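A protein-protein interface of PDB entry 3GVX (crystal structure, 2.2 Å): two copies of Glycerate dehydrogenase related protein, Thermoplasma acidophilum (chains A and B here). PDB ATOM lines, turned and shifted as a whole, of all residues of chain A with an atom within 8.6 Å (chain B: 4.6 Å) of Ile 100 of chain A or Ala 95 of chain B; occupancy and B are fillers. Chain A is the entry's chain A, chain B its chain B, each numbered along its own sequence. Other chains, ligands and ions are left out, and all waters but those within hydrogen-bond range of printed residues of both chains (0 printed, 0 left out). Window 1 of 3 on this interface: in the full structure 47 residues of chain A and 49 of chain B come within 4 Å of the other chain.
His 96 of chain A touches none of the printed residues of chain B.
Of the printed residues of chain B, Lys 98 of chain A touches His 88 (3.8 Å) and Ala 91 (3.5 Å).
Of the printed residues of chain B, Ile 100 of chain A touches Leu 92 (3.7 Å), Ala 95 (3.997 Å) and Ile 251 (3.99 Å).
Of the printed residues of chain A, Ala 95 of chain B touches Ile 100 (3.997 Å).
Of the printed residues of chain A, Leu 101 of chain B touches Leu 101 (3.7 Å) and Asn 104 (3.6 Å).
The nearest printed residue of chain A that does not touch Ala 95 of chain B is Ala 91 of chain A (4.9 Å).
The nearest printed residue of chain A that does not touch Ile 251 of chain B is Leu 101 of chain A (6.6 Å).
The backbone carbonyl oxygen (O) of Ala 95 of chain A is in hydrogen-bond range of the backbone NH (N) of Ile 100 of chain A, 2.9 Å away.
N of Ile 100 of chain B is in hydrogen-bond range of O of Ala 95 of chain B (2.9 Å).
Ala 91 of chain A touches Leu 94 of chain B.
Ala 91 of chain A touches Lys 98 of chain B (CB to CG, 3.4 Å).
CD1 of Ile 100 of chain B touches CD2 of Leu 92 of chain A, 3.6 Å away.
CB of Ala 91 of chain B touches CB of Leu 94 of chain A, at 3.6 Å.
ND1 of His 88 of chain B touches CB of Lys 98 of chain A (3.8 Å).
Leu 92 of chain B touches Ile 100 of chain A.
Ile 100 of chain A touches Ala 95 of chain B.
Ile 100 of chain A touches Ile 251 of chain B.
CD1 of Leu 101 of chain B touches CD1 of Leu 101 of chain A, at 3.7 Å.
OD1 of Asn 104 of chain A touches CD2 of Leu 101 of chain B (3.6 Å).
The side-chain carboxylate (OE1) of Glu 87 of chain A lies within salt-bridge range of the side-chain amino group (NZ) of Lys 98 of chain B.
His 88 of chain A touches Lys 98 of chain B, and with the chains exchanged Lys 98 of chain A touches His 88 of chain B.
Ala 91 of chain A touches Leu 94 of chain B, and with the chains exchanged Leu 94 of chain A touches Ala 91 of chain B.
Leu 92 of chain A touches Ile 100 of chain B, and with the chains exchanged Ile 100 of chain A touches Leu 92 of chain B.
Ile 100 of chain A touches Ile 251 of chain B, but with the chains exchanged Ile 251 of chain A does not touch Ile 100 of chain B (4.2 Å).
Hydrophobic or aromatic side chains of chain B within 4 Å of the printed part of chain A: His 88, Ala 91, Leu 92, Leu 94, Ala 95, Ile 100, Leu 101 and Ile 251.
Along chain B the printed residues that touch a printed residue of chain A span positions 88 to 251.
Hydrophobic or aromatic side chains of chain A that line the printed part of chain B: His 88, Ala 91, Leu 92, Leu 94, Ile 100 and Leu 101.
Among the printed residues, 15 pairs touch across the chains.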
ATOM      1  N   GLU A  87      10.506 -20.862  -9.545  1.00  0.00           N
ATOM      2  CA  GLU A  87       9.195 -20.255  -9.309  1.00  0.00           C
ATOM      3  C   GLU A  87       8.916 -19.260 -10.426  1.00  0.00           C
ATOM      4  O   GLU A  87       7.850 -19.249 -11.034  1.00  0.00           O
ATOM      5  CB  GLU A  87       9.119 -19.549  -7.941  1.00  0.00           C
ATOM      6  CG  GLU A  87       9.076 -20.501  -6.759  1.00  0.00           C
ATOM      7  CD  GLU A  87       8.691 -19.813  -5.438  1.00  0.00           C
ATOM      8  OE1 GLU A  87       8.246 -18.647  -5.475  1.00  0.00           O
ATOM      9  OE2 GLU A  87       8.824 -20.430  -4.360  1.00  0.00           O
ATOM     10  N   HIS A  88       9.925 -18.458 -10.718  1.00  0.00           N
ATOM     11  CA  HIS A  88       9.810 -17.451 -11.755  1.00  0.00           C
ATOM     12  C   HIS A  88       9.569 -18.008 -13.142  1.00  0.00           C
ATOM     13  O   HIS A  88       8.760 -17.468 -13.885  1.00  0.00           O
ATOM     14  CB  HIS A  88      11.049 -16.566 -11.787  1.00  0.00           C
ATOM     15  CG  HIS A  88      10.838 -15.292 -12.523  1.00  0.00           C
ATOM     16  ND1 HIS A  88      10.402 -14.140 -11.907  1.00  0.00           N
ATOM     17  CD2 HIS A  88      10.958 -14.990 -13.841  1.00  0.00           C
ATOM     18  CE1 HIS A  88      10.263 -13.186 -12.809  1.00  0.00           C
ATOM     19  NE2 HIS A  88      10.595 -13.675 -13.987  1.00  0.00           N
ATOM     20  N   PHE A  90       8.154 -20.781 -13.877  1.00  0.00           N
ATOM     21  CA  PHE A  90       6.786 -21.260 -13.922  1.00  0.00           C
ATOM     22  C   PHE A  90       5.763 -20.123 -13.928  1.00  0.00           C
ATOM     23  O   PHE A  90       4.676 -20.281 -14.482  1.00  0.00           O
ATOM     24  CB  PHE A  90       6.526 -22.254 -12.778  1.00  0.00           C
ATOM     25  CG  PHE A  90       6.691 -23.696 -13.196  1.00  0.00           C
ATOM     26  CD1 PHE A  90       5.681 -24.343 -13.903  1.00  0.00           C
ATOM     27  CD2 PHE A  90       7.890 -24.364 -12.996  1.00  0.00           C
ATOM     28  CE1 PHE A  90       5.870 -25.633 -14.419  1.00  0.00           C
ATOM     29  CE2 PHE A  90       8.089 -25.655 -13.510  1.00  0.00           C
ATOM     30  CZ  PHE A  90       7.077 -26.285 -14.223  1.00  0.00           C
ATOM     31  N   ALA A  91       6.112 -18.977 -13.345  1.00  0.00           N
ATOM     32  CA  ALA A  91       5.178 -17.852 -13.340  1.00  0.00           C
ATOM     33  C   ALA A  91       5.019 -17.327 -14.764  1.00  0.00           C
ATOM     34  O   ALA A  91       3.912 -17.043 -15.200  1.00  0.00           O
ATOM     35  CB  ALA A  91       5.662 -16.757 -12.410  1.00  0.00           C
ATOM     36  N   LEU A  92       6.128 -17.239 -15.498  1.00  0.00           N
ATOM     37  CA  LEU A  92       6.106 -16.787 -16.897  1.00  0.00           C
ATOM     38  C   LEU A  92       5.329 -17.778 -17.758  1.00  0.00           C
ATOM     39  O   LEU A  92       4.426 -17.424 -18.513  1.00  0.00           O
ATOM     40  CB  LEU A  92       7.530 -16.659 -17.464  1.00  0.00           C
ATOM     41  CG  LEU A  92       8.393 -15.495 -16.976  1.00  0.00           C
ATOM     42  CD1 LEU A  92       9.754 -15.546 -17.670  1.00  0.00           C
ATOM     43  CD2 LEU A  92       7.663 -14.179 -17.252  1.00  0.00           C
ATOM     44  N   LEU A  93       5.699 -19.039 -17.614  1.00  0.00           N
ATOM     45  CA  LEU A  93       5.074 -20.111 -18.363  1.00  0.00           C
ATOM     46  C   LEU A  93       3.564 -20.190 -18.136  1.00  0.00           C
ATOM     47  O   LEU A  93       2.812 -20.315 -19.076  1.00  0.00           O
ATOM     48  CB  LEU A  93       5.760 -21.436 -18.022  1.00  0.00           C
ATOM     49  CG  LEU A  93       5.563 -22.602 -18.989  1.00  0.00           C
ATOM     50  CD1 LEU A  93       6.617 -23.680 -18.702  1.00  0.00           C
ATOM     51  CD2 LEU A  93       4.142 -23.134 -18.861  1.00  0.00           C
ATOM     52  N   LEU A  94       3.125 -20.100 -16.889  1.00  0.00           N
ATOM     53  CA  LEU A  94       1.694 -20.160 -16.597  1.00  0.00           C
ATOM     54  C   LEU A  94       0.937 -18.918 -17.052  1.00  0.00           C
ATOM     55  O   LEU A  94      -0.215 -19.012 -17.451  1.00  0.00           O
ATOM     56  CB  LEU A  94       1.454 -20.374 -15.103  1.00  0.00           C
ATOM     57  CG  LEU A  94       1.775 -21.762 -14.557  1.00  0.00           C
ATOM     58  CD1 LEU A  94       1.702 -21.734 -13.035  1.00  0.00           C
ATOM     59  CD2 LEU A  94       0.798 -22.791 -15.155  1.00  0.00           C
ATOM     60  N   ALA A  95       1.591 -17.760 -16.991  1.00  0.00           N
ATOM     61  CA  ALA A  95       0.976 -16.497 -17.413  1.00  0.00           C
ATOM     62  C   ALA A  95       0.555 -16.609 -18.865  1.00  0.00           C
ATOM     63  O   ALA A  95      -0.512 -16.142 -19.243  1.00  0.00           O
ATOM     64  CB  ALA A  95       1.951 -15.338 -17.239  1.00  0.00           C
ATOM     65  N   HIS A  96       1.393 -17.256 -19.666  1.00  0.00           N
ATOM     66  CA  HIS A  96       1.095 -17.454 -21.070  1.00  0.00           C
ATOM     67  C   HIS A  96       0.134 -18.612 -21.298  1.00  0.00           C
ATOM     68  O   HIS A  96      -0.808 -18.489 -22.068  1.00  0.00           O
ATOM     69  CB  HIS A  96       2.382 -17.670 -21.878  1.00  0.00           C
ATOM     70  CG  HIS A  96       2.136 -18.020 -23.306  1.00  0.00           C
ATOM     71  ND1 HIS A  96       1.323 -17.269 -24.126  1.00  0.00           N
ATOM     72  CD2 HIS A  96       2.536 -19.081 -24.046  1.00  0.00           C
ATOM     73  CE1 HIS A  96       1.225 -17.855 -25.303  1.00  0.00           C
ATOM     74  NE2 HIS A  96       1.952 -18.956 -25.281  1.00  0.00           N
ATOM     75  N   ALA A  97       0.361 -19.733 -20.621  1.00  0.00           N
ATOM     76  CA  ALA A  97      -0.520 -20.887 -20.774  1.00  0.00           C
ATOM     77  C   ALA A  97      -1.963 -20.510 -20.473  1.00  0.00           C
ATOM     78  O   ALA A  97      -2.860 -20.887 -21.210  1.00  0.00           O
ATOM     79  CB  ALA A  97      -0.077 -22.035 -19.873  1.00  0.00           C
ATOM     80  N   LYS A  98      -2.184 -19.735 -19.414  1.00  0.00           N
ATOM     81  CA  LYS A  98      -3.535 -19.324 -19.058  1.00  0.00           C
ATOM     82  C   LYS A  98      -3.961 -17.961 -19.608  1.00  0.00           C
ATOM     83  O   LYS A  98      -5.000 -17.440 -19.209  1.00  0.00           O
ATOM     84  CB  LYS A  98      -3.722 -19.326 -17.536  1.00  0.00           C
ATOM     85  CG  LYS A  98      -3.246 -20.588 -16.843  1.00  0.00           C
ATOM     86  CD  LYS A  98      -3.662 -21.867 -17.560  1.00  0.00           C
ATOM     87  CE  LYS A  98      -3.235 -23.073 -16.731  1.00  0.00           C
ATOM     88  NZ  LYS A  98      -3.356 -24.396 -17.393  1.00  0.00           N
ATOM     89  N   ASN A  99      -3.163 -17.383 -20.504  1.00  0.00           N
ATOM     90  CA  ASN A  99      -3.493 -16.085 -21.094  1.00  0.00           C
ATOM     91  C   ASN A  99      -3.905 -15.107 -20.007  1.00  0.00           C
ATOM     92  O   ASN A  99      -4.891 -14.381 -20.143  1.00  0.00           O
ATOM     93  CB  ASN A  99      -4.661 -16.223 -22.077  1.00  0.00           C
ATOM     94  CG  ASN A  99      -4.418 -17.279 -23.132  1.00  0.00           C
ATOM     95  OD1 ASN A  99      -5.307 -18.079 -23.436  1.00  0.00           O
ATOM     96  ND2 ASN A  99      -3.219 -17.293 -23.697  1.00  0.00           N
ATOM     97  N   ILE A 100      -3.155 -15.096 -18.918  1.00  0.00           N
ATOM     98  CA  ILE A 100      -3.456 -14.239 -17.786  1.00  0.00           C
ATOM     99  C   ILE A 100      -3.476 -12.757 -18.124  1.00  0.00           C
ATOM    100  O   ILE A 100      -4.331 -12.024 -17.644  1.00  0.00           O
ATOM    101  CB  ILE A 100      -2.453 -14.473 -16.633  1.00  0.00           C
ATOM    102  CG1 ILE A 100      -2.616 -15.891 -16.078  1.00  0.00           C
ATOM    103  CG2 ILE A 100      -2.627 -13.419 -15.552  1.00  0.00           C
ATOM    104  CD1 ILE A 100      -3.935 -16.171 -15.406  1.00  0.00           C
ATOM    105  N   LEU A 101      -2.543 -12.303 -18.950  1.00  0.00           N
ATOM    106  CA  LEU A 101      -2.503 -10.884 -19.288  1.00  0.00           C
ATOM    107  C   LEU A 101      -3.664 -10.427 -20.148  1.00  0.00           C
ATOM    108  O   LEU A 101      -4.333  -9.449 -19.841  1.00  0.00           O
ATOM    109  CB  LEU A 101      -1.191 -10.525 -19.990  1.00  0.00           C
ATOM    110  CG  LEU A 101       0.056 -10.264 -19.146  1.00  0.00           C
ATOM    111  CD1 LEU A 101       0.400 -11.487 -18.281  1.00  0.00           C
ATOM    112  CD2 LEU A 101       1.188  -9.881 -20.105  1.00  0.00           C
ATOM    113  N   GLU A 102      -3.891 -11.142 -21.235  1.00  0.00           N
ATOM    114  CA  GLU A 102      -4.965 -10.781 -22.134  1.00  0.00           C
ATOM    115  C   GLU A 102      -6.328 -10.830 -21.468  1.00  0.00           C
ATOM    116  O   GLU A 102      -7.126  -9.914 -21.623  1.00  0.00           O
ATOM    117  CB  GLU A 102      -4.922 -11.670 -23.376  1.00  0.00           C
ATOM    118  CG  GLU A 102      -3.562 -11.658 -24.073  1.00  0.00           C
ATOM    119  CD  GLU A 102      -2.619 -12.775 -23.596  1.00  0.00           C
ATOM    120  OE1 GLU A 102      -2.754 -13.251 -22.445  1.00  0.00           O
ATOM    121  OE2 GLU A 102      -1.738 -13.178 -24.380  1.00  0.00           O
ATOM    122  N   ASN A 103      -6.597 -11.878 -20.704  1.00  0.00           N
ATOM    123  CA  ASN A 103      -7.884 -11.965 -20.037  1.00  0.00           C
ATOM    124  C   ASN A 103      -8.065 -10.927 -18.942  1.00  0.00           C
ATOM    125  O   ASN A 103      -9.141 -10.376 -18.787  1.00  0.00           O
ATOM    126  CB  ASN A 103      -8.122 -13.374 -19.488  1.00  0.00           C
ATOM    127  CG  ASN A 103      -8.289 -14.385 -20.582  1.00  0.00           C
ATOM    128  OD1 ASN A 103      -8.511 -14.025 -21.736  1.00  0.00           O
ATOM    129  ND2 ASN A 103      -8.186 -15.664 -20.231  1.00  0.00           N
ATOM    130  N   ASN A 104      -7.002 -10.651 -18.198  1.00  0.00           N
ATOM    131  CA  ASN A 104      -7.097  -9.670 -17.135  1.00  0.00           C
ATOM    132  C   ASN A 104      -7.467  -8.322 -17.694  1.00  0.00           C
ATOM    133  O   ASN A 104      -8.312  -7.633 -17.135  1.00  0.00           O
ATOM    134  CB  ASN A 104      -5.795  -9.530 -16.351  1.00  0.00           C
ATOM    135  CG  ASN A 104      -5.855  -8.413 -15.328  1.00  0.00           C
ATOM    136  OD1 ASN A 104      -5.118  -7.422 -15.417  1.00  0.00           O
ATOM    137  ND2 ASN A 104      -6.738  -8.567 -14.342  1.00  0.00           N
ATOM    138  N   GLU A 105      -6.826  -7.945 -18.792  1.00  0.00           N
ATOM    139  CA  GLU A 105      -7.082  -6.668 -19.446  1.00  0.00           C
ATOM    140  C   GLU A 105      -8.542  -6.548 -19.846  1.00  0.00           C
ATOM    141  O   GLU A 105      -9.193  -5.531 -19.599  1.00  0.00           O
ATOM    142  CB  GLU A 105      -6.232  -6.540 -20.697  1.00  0.00           C
ATOM    143  CG  GLU A 105      -6.170  -5.144 -21.217  1.00  0.00           C
ATOM    144  CD  GLU A 105      -4.940  -4.937 -22.053  1.00  0.00           C
ATOM    145  OE1 GLU A 105      -4.988  -5.242 -23.264  1.00  0.00           O
ATOM    146  OE2 GLU A 105      -3.916  -4.489 -21.486  1.00  0.00           O
ATOM    147  N   LEU A 106      -9.034  -7.600 -20.487  1.00  0.00           N
ATOM    148  CA  LEU A 106     -10.417  -7.656 -20.924  1.00  0.00           C
ATOM    149  C   LEU A 106     -11.348  -7.530 -19.756  1.00  0.00           C
ATOM    150  O   LEU A 106     -12.198  -6.648 -19.710  1.00  0.00           O
ATOM    151  CB  LEU A 106     -10.718  -8.970 -21.629  1.00  0.00           C
ATOM    152  CG  LEU A 106     -10.287  -9.062 -23.083  1.00  0.00           C
ATOM    153  CD1 LEU A 106     -10.732 -10.419 -23.632  1.00  0.00           C
ATOM    154  CD2 LEU A 106     -10.878  -7.888 -23.874  1.00  0.00           C
ATOM    155  N   MET A 107     -11.181  -8.427 -18.801  1.00  0.00           N
ATOM    156  CA  MET A 107     -12.038  -8.410 -17.649  1.00  0.00           C
ATOM    157  C   MET A 107     -12.060  -7.063 -16.956  1.00  0.00           C
ATOM    158  O   MET A 107     -13.094  -6.671 -16.465  1.00  0.00           O
ATOM    159  CB  MET A 107     -11.671  -9.558 -16.714  1.00  0.00           C
ATOM    160  CG  MET A 107     -12.104 -10.925 -17.250  1.00  0.00           C
ATOM    161  SD  MET A 107     -13.762 -11.390 -16.746  1.00  0.00           S
ATOM    162  CE  MET A 107     -13.910 -10.599 -15.179  1.00  0.00           C
ATOM    163  N   PRO A 116     -10.094 -20.659 -24.364  1.00  0.00           N
ATOM    164  CA  PRO A 116      -9.419 -21.831 -23.822  1.00  0.00           C
ATOM    165  C   PRO A 116      -8.018 -21.468 -23.363  1.00  0.00           C
ATOM    166  O   PRO A 116      -7.423 -20.494 -23.824  1.00  0.00           O
ATOM    167  CB  PRO A 116      -9.396 -22.793 -25.006  1.00  0.00           C
ATOM    168  CG  PRO A 116      -9.286 -21.853 -26.169  1.00  0.00           C
ATOM    169  CD  PRO A 116     -10.300 -20.798 -25.813  1.00  0.00           C
ATOM    170  N   THR A 117      -7.517 -22.260 -22.431  1.00  0.00           N
ATOM    171  CA  THR A 117      -6.190 -22.061 -21.918  1.00  0.00           C
ATOM    172  C   THR A 117      -5.448 -23.347 -22.180  1.00  0.00           C
ATOM    173  O   THR A 117      -6.052 -24.385 -22.436  1.00  0.00           O
ATOM    174  CB  THR A 117      -6.213 -21.744 -20.409  1.00  0.00           C
ATOM    175  OG1 THR A 117      -6.824 -22.828 -19.700  1.00  0.00           O
ATOM    176  CG2 THR A 117      -6.976 -20.447 -20.144  1.00  0.00           C
ATOM    177  N   ILE A 251       6.868 -12.369 -23.240  1.00  0.00           N
ATOM    178  CA  ILE A 251       6.525 -11.857 -21.936  1.00  0.00           C
ATOM    179  C   ILE A 251       7.882 -11.691 -21.330  1.00  0.00           C
ATOM    180  O   ILE A 251       8.731 -12.589 -21.400  1.00  0.00           O
ATOM    181  CB  ILE A 251       5.690 -12.813 -21.085  1.00  0.00           C
ATOM    182  CG1 ILE A 251       4.400 -13.175 -21.807  1.00  0.00           C
ATOM    183  CG2 ILE A 251       5.377 -12.137 -19.768  1.00  0.00           C
ATOM    184  CD1 ILE A 251       3.416 -13.934 -20.959  1.00  0.00           C
ATOM    185  N   HIS B  88      -4.738 -23.183 -12.858  1.00  0.00           N
ATOM    186  CA  HIS B  88      -5.142 -21.809 -13.105  1.00  0.00           C
ATOM    187  C   HIS B  88      -4.938 -20.962 -11.866  1.00  0.00           C
ATOM    188  O   HIS B  88      -4.626 -19.781 -11.964  1.00  0.00           O
ATOM    189  CB  HIS B  88      -6.609 -21.711 -13.521  1.00  0.00           C
ATOM    190  CG  HIS B  88      -6.987 -20.359 -14.020  1.00  0.00           C
ATOM    191  ND1 HIS B  88      -6.784 -19.965 -15.319  1.00  0.00           N
ATOM    192  CD2 HIS B  88      -7.485 -19.274 -13.375  1.00  0.00           C
ATOM    193  CE1 HIS B  88      -7.137 -18.701 -15.460  1.00  0.00           C
ATOM    194  NE2 HIS B  88      -7.564 -18.260 -14.293  1.00  0.00           N
ATOM    195  N   ALA B  91      -1.394 -20.048 -11.544  1.00  0.00           N
ATOM    196  CA  ALA B  91      -1.067 -19.078 -12.581  1.00  0.00           C
ATOM    197  C   ALA B  91      -1.379 -17.654 -12.108  1.00  0.00           C
ATOM    198  O   ALA B  91      -0.596 -16.729 -12.337  1.00  0.00           O
ATOM    199  CB  ALA B  91      -1.824 -19.399 -13.872  1.00  0.00           C
ATOM    200  N   LEU B  92      -2.512 -17.484 -11.428  1.00  0.00           N
ATOM    201  CA  LEU B  92      -2.894 -16.169 -10.898  1.00  0.00           C
ATOM    202  C   LEU B  92      -1.963 -15.788  -9.772  1.00  0.00           C
ATOM    203  O   LEU B  92      -1.461 -14.672  -9.676  1.00  0.00           O
ATOM    204  CB  LEU B  92      -4.317 -16.205 -10.361  1.00  0.00           C
ATOM    205  CG  LEU B  92      -5.325 -16.329 -11.483  1.00  0.00           C
ATOM    206  CD1 LEU B  92      -6.680 -16.743 -10.922  1.00  0.00           C
ATOM    207  CD2 LEU B  92      -5.351 -15.006 -12.248  1.00  0.00           C
ATOM    208  N   LEU B  93      -1.772 -16.766  -8.904  1.00  0.00           N
ATOM    209  CA  LEU B  93      -0.922 -16.660  -7.737  1.00  0.00           C
ATOM    210  C   LEU B  93       0.474 -16.155  -8.094  1.00  0.00           C
ATOM    211  O   LEU B  93       0.956 -15.178  -7.521  1.00  0.00           O
ATOM    212  CB  LEU B  93      -0.827 -18.026  -7.083  1.00  0.00           C
ATOM    213  CG  LEU B  93      -0.877 -18.002  -5.560  1.00  0.00           C
ATOM    214  CD1 LEU B  93      -1.338 -19.373  -5.078  1.00  0.00           C
ATOM    215  CD2 LEU B  93       0.471 -17.579  -4.986  1.00  0.00           C
ATOM    216  N   LEU B  94       1.110 -16.830  -9.047  1.00  0.00           N
ATOM    217  CA  LEU B  94       2.452 -16.462  -9.493  1.00  0.00           C
ATOM    218  C   LEU B  94       2.491 -15.173 -10.318  1.00  0.00           C
ATOM    219  O   LEU B  94       3.488 -14.470 -10.315  1.00  0.00           O
ATOM    220  CB  LEU B  94       3.079 -17.624 -10.273  1.00  0.00           C
ATOM    221  CG  LEU B  94       3.395 -18.844  -9.408  1.00  0.00           C
ATOM    222  CD1 LEU B  94       3.672 -20.049 -10.299  1.00  0.00           C
ATOM    223  CD2 LEU B  94       4.574 -18.529  -8.498  1.00  0.00           C
ATOM    224  N   ALA B  95       1.400 -14.869 -11.015  1.00  0.00           N
ATOM    225  CA  ALA B  95       1.339 -13.648 -11.817  1.00  0.00           C
ATOM    226  C   ALA B  95       1.543 -12.466 -10.893  1.00  0.00           C
ATOM    227  O   ALA B  95       2.302 -11.563 -11.187  1.00  0.00           O
ATOM    228  CB  ALA B  95      -0.009 -13.531 -12.534  1.00  0.00           C
ATOM    229  N   HIS B  96       0.857 -12.509  -9.762  1.00  0.00           N
ATOM    230  CA  HIS B  96       0.958 -11.463  -8.751  1.00  0.00           C
ATOM    231  C   HIS B  96       2.261 -11.530  -7.962  1.00  0.00           C
ATOM    232  O   HIS B  96       2.922 -10.520  -7.778  1.00  0.00           O
ATOM    233  CB  HIS B  96      -0.240 -11.533  -7.789  1.00  0.00           C
ATOM    234  CG  HIS B  96      -0.142 -10.586  -6.641  1.00  0.00           C
ATOM    235  ND1 HIS B  96       0.117  -9.246  -6.804  1.00  0.00           N
ATOM    236  CD2 HIS B  96      -0.232 -10.792  -5.304  1.00  0.00           C
ATOM    237  CE1 HIS B  96       0.189  -8.666  -5.619  1.00  0.00           C
ATOM    238  NE2 HIS B  96      -0.019  -9.584  -4.693  1.00  0.00           N
ATOM    239  N   ALA B  97       2.641 -12.722  -7.518  1.00  0.00           N
ATOM    240  CA  ALA B  97       3.866 -12.871  -6.752  1.00  0.00           C
ATOM    241  C   ALA B  97       5.112 -12.383  -7.477  1.00  0.00           C
ATOM    242  O   ALA B  97       5.967 -11.782  -6.862  1.00  0.00           O
ATOM    243  CB  ALA B  97       4.044 -14.322  -6.297  1.00  0.00           C
ATOM    244  N   LYS B  98       5.200 -12.611  -8.783  1.00  0.00           N
ATOM    245  CA  LYS B  98       6.373 -12.185  -9.555  1.00  0.00           C
ATOM    246  C   LYS B  98       6.174 -10.863 -10.297  1.00  0.00           C
ATOM    247  O   LYS B  98       6.968 -10.496 -11.167  1.00  0.00           O
ATOM    248  CB  LYS B  98       6.786 -13.288 -10.554  1.00  0.00           C
ATOM    249  CG  LYS B  98       6.808 -14.679  -9.946  1.00  0.00           C
ATOM    250  CD  LYS B  98       7.751 -14.755  -8.747  1.00  0.00           C
ATOM    251  CE  LYS B  98       7.729 -16.133  -8.112  1.00  0.00           C
ATOM    252  NZ  LYS B  98       8.673 -16.273  -6.966  1.00  0.00           N
ATOM    253  N   ASN B  99       5.090 -10.174  -9.951  1.00  0.00           N
ATOM    254  CA  ASN B  99       4.770  -8.899 -10.583  1.00  0.00           C
ATOM    255  C   ASN B  99       4.921  -9.035 -12.084  1.00  0.00           C
ATOM    256  O   ASN B  99       5.526  -8.200 -12.746  1.00  0.00           O
ATOM    257  CB  ASN B  99       5.702  -7.805 -10.056  1.00  0.00           C
ATOM    258  CG  ASN B  99       5.556  -7.596  -8.565  1.00  0.00           C
ATOM    259  OD1 ASN B  99       6.546  -7.384  -7.856  1.00  0.00           O
ATOM    260  ND2 ASN B  99       4.320  -7.642  -8.075  1.00  0.00           N
ATOM    261  N   ILE B 100       4.374 -10.112 -12.621  1.00  0.00           N
ATOM    262  CA  ILE B 100       4.474 -10.389 -14.041  1.00  0.00           C
ATOM    263  C   ILE B 100       3.913  -9.292 -14.958  1.00  0.00           C
ATOM    264  O   ILE B 100       4.598  -8.860 -15.879  1.00  0.00           O
ATOM    265  CB  ILE B 100       3.807 -11.746 -14.384  1.00  0.00           C
ATOM    266  CG1 ILE B 100       4.586 -12.887 -13.722  1.00  0.00           C
ATOM    267  CG2 ILE B 100       3.705 -11.928 -15.894  1.00  0.00           C
ATOM    268  CD1 ILE B 100       6.026 -13.046 -14.205  1.00  0.00           C
ATOM    269  N   LEU B 101       2.687  -8.834 -14.713  1.00  0.00           N
ATOM    270  CA  LEU B 101       2.073  -7.808 -15.570  1.00  0.00           C
ATOM    271  C   LEU B 101       2.797  -6.461 -15.585  1.00  0.00           C
ATOM    272  O   LEU B 101       3.054  -5.886 -16.641  1.00  0.00           O
ATOM    273  CB  LEU B 101       0.618  -7.571 -15.163  1.00  0.00           C
ATOM    274  CG  LEU B 101      -0.502  -8.596 -15.365  1.00  0.00           C
ATOM    275  CD1 LEU B 101      -0.062  -9.996 -14.967  1.00  0.00           C
ATOM    276  CD2 LEU B 101      -1.714  -8.101 -14.560  1.00  0.00           C
ATOM    277  N   ILE B 251      -6.329  -9.281 -10.085  1.00  0.00           N
ATOM    278  CA  ILE B 251      -6.027  -9.866 -11.377  1.00  0.00           C
ATOM    279  C   ILE B 251      -7.229 -10.766 -11.545  1.00  0.00           C
ATOM    280  O   ILE B 251      -7.569 -11.557 -10.661  1.00  0.00           O
ATOM    281  CB  ILE B 251      -4.753 -10.725 -11.383  1.00  0.00           C
ATOM    282  CG1 ILE B 251      -3.556  -9.909 -10.905  1.00  0.00           C
ATOM    283  CG2 ILE B 251      -4.503 -11.245 -12.787  1.00  0.00           C
ATOM    284  CD1 ILE B 251      -2.242 -10.640 -11.002  1.00  0.00           C
